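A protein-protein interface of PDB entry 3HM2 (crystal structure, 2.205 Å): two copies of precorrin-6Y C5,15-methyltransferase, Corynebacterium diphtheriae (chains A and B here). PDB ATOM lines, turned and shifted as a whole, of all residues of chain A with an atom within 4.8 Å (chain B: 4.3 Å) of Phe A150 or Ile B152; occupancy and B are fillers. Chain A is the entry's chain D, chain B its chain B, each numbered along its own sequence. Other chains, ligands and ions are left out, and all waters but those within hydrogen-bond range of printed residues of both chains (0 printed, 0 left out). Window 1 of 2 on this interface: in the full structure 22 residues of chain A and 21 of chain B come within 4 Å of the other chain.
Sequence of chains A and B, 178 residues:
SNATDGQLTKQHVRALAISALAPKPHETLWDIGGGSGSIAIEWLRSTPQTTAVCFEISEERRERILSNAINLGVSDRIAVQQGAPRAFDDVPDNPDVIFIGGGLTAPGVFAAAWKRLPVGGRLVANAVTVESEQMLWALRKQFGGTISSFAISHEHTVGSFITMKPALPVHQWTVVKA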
ATOM      1  N   LEU A  16      -7.257   2.908  -6.913  1.00  0.00           N
ATOM      2  CA  LEU A  16      -6.264   2.520  -7.937  1.00  0.00           C
ATOM      3  C   LEU A  16      -6.868   1.863  -9.183  1.00  0.00           C
ATOM      4  O   LEU A  16      -6.523   2.208 -10.321  1.00  0.00           O
ATOM      5  CB  LEU A  16      -5.199   1.610  -7.327  1.00  0.00           C
ATOM      6  CG  LEU A  16      -4.231   2.426  -6.475  1.00  0.00           C
ATOM      7  CD1 LEU A  16      -3.527   1.547  -5.455  1.00  0.00           C
ATOM      8  CD2 LEU A  16      -3.240   3.195  -7.358  1.00  0.00           C
ATOM      9  N   SER A 148       1.933  -3.667 -12.700  1.00  0.00           N
ATOM     10  CA  SER A 148       2.439  -2.746 -11.689  1.00  0.00           C
ATOM     11  C   SER A 148       2.045  -3.411 -10.399  1.00  0.00           C
ATOM     12  O   SER A 148       1.167  -4.266 -10.408  1.00  0.00           O
ATOM     13  CB  SER A 148       1.707  -1.392 -11.729  1.00  0.00           C
ATOM     14  OG  SER A 148       2.017  -0.612 -12.876  1.00  0.00           O
ATOM     15  N   SER A 149       2.682  -3.032  -9.297  1.00  0.00           N
ATOM     16  CA  SER A 149       2.251  -3.500  -7.985  1.00  0.00           C
ATOM     17  C   SER A 149       2.457  -2.393  -6.956  1.00  0.00           C
ATOM     18  O   SER A 149       3.408  -1.600  -7.051  1.00  0.00           O
ATOM     19  CB  SER A 149       2.988  -4.769  -7.557  1.00  0.00           C
ATOM     20  OG  SER A 149       4.317  -4.468  -7.171  1.00  0.00           O
ATOM     21  N   PHE A 150       1.551  -2.373  -5.978  1.00  0.00           N
ATOM     22  CA  PHE A 150       1.442  -1.333  -4.967  1.00  0.00           C
ATOM     23  C   PHE A 150       1.623  -1.938  -3.554  1.00  0.00           C
ATOM     24  O   PHE A 150       0.894  -2.855  -3.173  1.00  0.00           O
ATOM     25  CB  PHE A 150       0.065  -0.643  -5.122  1.00  0.00           C
ATOM     26  CG  PHE A 150      -0.378  -0.490  -6.564  1.00  0.00           C
ATOM     27  CD1 PHE A 150       0.018   0.615  -7.325  1.00  0.00           C
ATOM     28  CD2 PHE A 150      -1.168  -1.467  -7.172  1.00  0.00           C
ATOM     29  CE1 PHE A 150      -0.356   0.735  -8.659  1.00  0.00           C
ATOM     30  CE2 PHE A 150      -1.560  -1.345  -8.506  1.00  0.00           C
ATOM     31  CZ  PHE A 150      -1.155  -0.244  -9.245  1.00  0.00           C
ATOM     32  N   ALA A 151       2.608  -1.451  -2.792  1.00  0.00           N
ATOM     33  CA  ALA A 151       2.821  -1.925  -1.426  1.00  0.00           C
ATOM     34  C   ALA A 151       2.304  -0.918  -0.398  1.00  0.00           C
ATOM     35  O   ALA A 151       3.022  -0.013   0.055  1.00  0.00           O
ATOM     36  CB  ALA A 151       4.284  -2.241  -1.183  1.00  0.00           C
ATOM     37  N   ILE A 152       1.038  -1.079  -0.027  1.00  0.00           N
ATOM     38  CA  ILE A 152       0.372  -0.131   0.857  1.00  0.00           C
ATOM     39  C   ILE A 152       0.462  -0.576   2.312  1.00  0.00           C
ATOM     40  O   ILE A 152       0.065  -1.689   2.657  1.00  0.00           O
ATOM     41  CB  ILE A 152      -1.110   0.049   0.476  1.00  0.00           C
ATOM     42  CG1 ILE A 152      -1.231   0.756  -0.875  1.00  0.00           C
ATOM     43  CG2 ILE A 152      -1.846   0.827   1.557  1.00  0.00           C
ATOM     44  CD1 ILE A 152      -0.184   0.332  -1.882  1.00  0.00           C
ATOM     45  N   PRO A 169       0.032  -7.050  -0.865  1.00  0.00           N
ATOM     46  CA  PRO A 169       0.353  -6.372  -2.135  1.00  0.00           C
ATOM     47  C   PRO A 169      -0.569  -6.732  -3.329  1.00  0.00           C
ATOM     48  O   PRO A 169      -0.871  -7.911  -3.535  1.00  0.00           O
ATOM     49  CB  PRO A 169       1.808  -6.816  -2.423  1.00  0.00           C
ATOM     50  CG  PRO A 169       2.305  -7.507  -1.148  1.00  0.00           C
ATOM     51  CD  PRO A 169       1.062  -8.051  -0.508  1.00  0.00           C
ATOM     52  N   VAL A 170      -1.000  -5.730  -4.104  1.00  0.00           N
ATOM     53  CA  VAL A 170      -1.765  -5.987  -5.325  1.00  0.00           C
ATOM     54  C   VAL A 170      -0.966  -5.837  -6.605  1.00  0.00           C
ATOM     55  O   VAL A 170      -0.286  -4.837  -6.850  1.00  0.00           O
ATOM     56  CB  VAL A 170      -2.987  -5.093  -5.467  1.00  0.00           C
ATOM     57  CG1 VAL A 170      -3.769  -5.469  -6.748  1.00  0.00           C
ATOM     58  CG2 VAL A 170      -3.853  -5.201  -4.241  1.00  0.00           C
ATOM     59  N   GLN A 172      -1.586  -5.354 -10.329  1.00  0.00           N
ATOM     60  CA  GLN A 172      -2.635  -4.938 -11.205  1.00  0.00           C
ATOM     61  C   GLN A 172      -2.236  -5.079 -12.665  1.00  0.00           C
ATOM     62  O   GLN A 172      -1.272  -4.481 -13.136  1.00  0.00           O
ATOM     63  CB  GLN A 172      -2.974  -3.506 -10.881  1.00  0.00           C
ATOM     64  CG  GLN A 172      -3.945  -2.926 -11.831  1.00  0.00           C
ATOM     65  CD  GLN A 172      -4.579  -1.694 -11.284  1.00  0.00           C
ATOM     66  OE1 GLN A 172      -4.093  -0.582 -11.508  1.00  0.00           O
ATOM     67  NE2 GLN A 172      -5.665  -1.875 -10.541  1.00  0.00           N
ATOM     68  N   HIS B  12      -0.562   6.898 -10.796  1.00  0.00           N
ATOM     69  CA  HIS B  12      -1.014   6.159  -9.612  1.00  0.00           C
ATOM     70  C   HIS B  12      -1.031   6.990  -8.316  1.00  0.00           C
ATOM     71  O   HIS B  12      -1.924   6.832  -7.461  1.00  0.00           O
ATOM     72  CB  HIS B  12      -0.191   4.872  -9.441  1.00  0.00           C
ATOM     73  CG  HIS B  12      -0.458   3.835 -10.497  1.00  0.00           C
ATOM     74  ND1 HIS B  12      -1.733   3.490 -10.904  1.00  0.00           N
ATOM     75  CD2 HIS B  12       0.387   3.053 -11.211  1.00  0.00           C
ATOM     76  CE1 HIS B  12      -1.658   2.553 -11.833  1.00  0.00           C
ATOM     77  NE2 HIS B  12      -0.384   2.270 -12.038  1.00  0.00           N
ATOM     78  N   PHE B 150       3.119   4.296   0.353  1.00  0.00           N
ATOM     79  CA  PHE B 150       2.966   3.706  -0.959  1.00  0.00           C
ATOM     80  C   PHE B 150       4.273   3.378  -1.672  1.00  0.00           C
ATOM     81  O   PHE B 150       4.974   4.271  -2.149  1.00  0.00           O
ATOM     82  CB  PHE B 150       2.088   4.590  -1.840  1.00  0.00           C
ATOM     83  CG  PHE B 150       0.859   5.094  -1.149  1.00  0.00           C
ATOM     84  CD1 PHE B 150       0.753   6.426  -0.782  1.00  0.00           C
ATOM     85  CD2 PHE B 150      -0.192   4.238  -0.867  1.00  0.00           C
ATOM     86  CE1 PHE B 150      -0.390   6.897  -0.141  1.00  0.00           C
ATOM     87  CE2 PHE B 150      -1.336   4.694  -0.226  1.00  0.00           C
ATOM     88  CZ  PHE B 150      -1.436   6.026   0.139  1.00  0.00           C
ATOM     89  N   ALA B 151       4.585   2.082  -1.736  1.00  0.00           N
ATOM     90  CA  ALA B 151       5.603   1.569  -2.649  1.00  0.00           C
ATOM     91  C   ALA B 151       4.919   1.055  -3.908  1.00  0.00           C
ATOM     92  O   ALA B 151       4.194   0.070  -3.864  1.00  0.00           O
ATOM     93  CB  ALA B 151       6.411   0.457  -1.995  1.00  0.00           C
ATOM     94  N   ILE B 152       5.151   1.732  -5.025  1.00  0.00           N
ATOM     95  CA  ILE B 152       4.553   1.344  -6.306  1.00  0.00           C
ATOM     96  C   ILE B 152       5.581   0.825  -7.325  1.00  0.00           C
ATOM     97  O   ILE B 152       6.531   1.530  -7.685  1.00  0.00           O
ATOM     98  CB  ILE B 152       3.720   2.510  -6.916  1.00  0.00           C
ATOM     99  CG1 ILE B 152       2.517   2.821  -6.012  1.00  0.00           C
ATOM    100  CG2 ILE B 152       3.324   2.216  -8.386  1.00  0.00           C
ATOM    101  CD1 ILE B 152       1.480   3.734  -6.630  1.00  0.00           C
ATOM    102  N   SER B 153       5.369  -0.405  -7.791  1.00  0.00           N
ATOM    103  CA  SER B 153       6.324  -1.061  -8.677  1.00  0.00           C
ATOM    104  C   SER B 153       5.802  -1.246 -10.105  1.00  0.00           C
ATOM    105  O   SER B 153       4.614  -1.474 -10.322  1.00  0.00           O
ATOM    106  CB  SER B 153       6.766  -2.404  -8.075  1.00  0.00           C
ATOM    107  OG  SER B 153       7.425  -2.211  -6.834  1.00  0.00           O
ATOM    108  N   HIS B 154       6.709  -1.133 -11.069  1.00  0.00           N
ATOM    109  CA  HIS B 154       6.383  -1.215 -12.473  1.00  0.00           C
ATOM    110  C   HIS B 154       7.285  -2.266 -13.077  1.00  0.00           C
ATOM    111  O   HIS B 154       8.475  -2.325 -12.773  1.00  0.00           O
ATOM    112  CB  HIS B 154       6.672   0.113 -13.193  1.00  0.00           C
ATOM    113  CG  HIS B 154       6.089   1.334 -12.539  1.00  0.00           C
ATOM    114  ND1 HIS B 154       4.768   1.706 -12.688  1.00  0.00           N
ATOM    115  CD2 HIS B 154       6.668   2.299 -11.782  1.00  0.00           C
ATOM    116  CE1 HIS B 154       4.551   2.825 -12.017  1.00  0.00           C
ATOM    117  NE2 HIS B 154       5.688   3.206 -11.461  1.00  0.00           N
ATOM    118  N   LYS B 165      10.405  -3.262 -10.741  1.00  0.00           N
ATOM    119  CA  LYS B 165      11.210  -2.166 -10.208  1.00  0.00           C
ATOM    120  C   LYS B 165      10.432  -1.212  -9.295  1.00  0.00           C
ATOM    121  O   LYS B 165       9.434  -0.620  -9.700  1.00  0.00           O
ATOM    122  CB  LYS B 165      11.895  -1.401 -11.346  1.00  0.00           C
ATOM    123  CG  LYS B 165      13.206  -0.730 -10.892  1.00  0.00           C
ATOM    124  CD  LYS B 165      13.918   0.061 -12.007  1.00  0.00           C
ATOM    125  CE  LYS B 165      15.025   0.976 -11.435  1.00  0.00           C
ATOM    126  NZ  LYS B 165      15.886   1.659 -12.467  1.00  0.00           N
ATOM    127  N   PRO B 166      10.900  -1.045  -8.051  1.00  0.00           N
ATOM    128  CA  PRO B 166      10.186  -0.206  -7.076  1.00  0.00           C
ATOM    129  C   PRO B 166      10.381   1.302  -7.294  1.00  0.00           C
ATOM    130  O   PRO B 166      11.526   1.756  -7.400  1.00  0.00           O
ATOM    131  CB  PRO B 166      10.837  -0.594  -5.728  1.00  0.00           C
ATOM    132  CG  PRO B 166      11.923  -1.605  -6.041  1.00  0.00           C
ATOM    133  CD  PRO B 166      12.173  -1.556  -7.514  1.00  0.00           C
ATOM    134  N   ALA B 167       9.298   2.076  -7.319  1.00  0.00           N
ATOM    135  CA  ALA B 167       9.459   3.529  -7.171  1.00  0.00           C
ATOM    136  C   ALA B 167       9.928   3.874  -5.748  1.00  0.00           C
ATOM    137  O   ALA B 167       9.892   3.029  -4.840  1.00  0.00           O
ATOM    138  CB  ALA B 167       8.161   4.280  -7.503  1.00  0.00           C
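The backbone carbonyl oxygen (O) of Ala B151 is in hydrogen-bond range of the backbone NH (N) of Ala A151. N of Ser B153 lies within hydrogen-bond range of O of Ser A149 (2.4 Å).
N of Phe A150 lies within hydrogen-bond range of O of Val A170, 3.2 Å away. N of Gln A172 is in hydrogen-bond range of O of Ser A148, 3.0 Å away. O of Ile B152 sits at hydrogen-bond distance from N of Ala B167. The backbone carbonyl oxygen (O) of His B154 lies within hydrogen-bond range of the backbone NH (N) of Lys B165.
Among the printed residues, pairs that only touch across the chains: Ser A148 with Ser B153, Ser A149 with Ile B152, Phe A150 with Ala B151, Phe A150 with Ile B152, Phe A150 with His B12, Ser A148 with His B154, Ile A152 with Phe B150, Ser A149 with Ala B151, Ser A148 with His B12, Ala A151 with Phe B150, Leu A16 with His B12 and Gln A172 with His B12.
Phe A150 touches three residues of chain B. Ile B152 touches just these residues of chain A: Ser A149 and Phe A150. Printed residues of chain B within 4 Å of Gln A172: His B12 (3.98 Å). Of the printed residues of chain A, His B12 touches Leu A16 (3.9 Å), Ser A148 (3.8 Å), Phe A150 (3.5 Å) and Gln A172 (3.98 Å). Of the printed residues of chain B, Ile A152 touches Phe B150. The nearest printed residue of chain B that does not touch Phe A150 is Ser B153 (4.7 Å). The nearest residue of chain A that does not touch Ile B152 is Ala A151 (4.6 Å). The nearest printed residue of chain A that does not touch Ala B151 is Ile A152 (4.8 Å).
Hydrophobic or aromatic side chains of chain B that line the printed part of chain A: His B12, Phe B150, Ala B151, Ile B152 and His B154. Of the 9 printed residues of chain A, 7 touch a printed residue of chain B.
Phe A150 touches Ala B151, and with the chains exchanged Ala A151 touches Phe B150. Phe A150 touches Ile B152, and with the chains exchanged Ile A152 touches Phe B150. Ala B151 touches its own counterpart, Ala A151. Positions printed for both chains: 150, 151 and 152. Of the 14 pairs that touch across the chains among the printed residues, 5 have their exchanged pair printed and touching as well.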
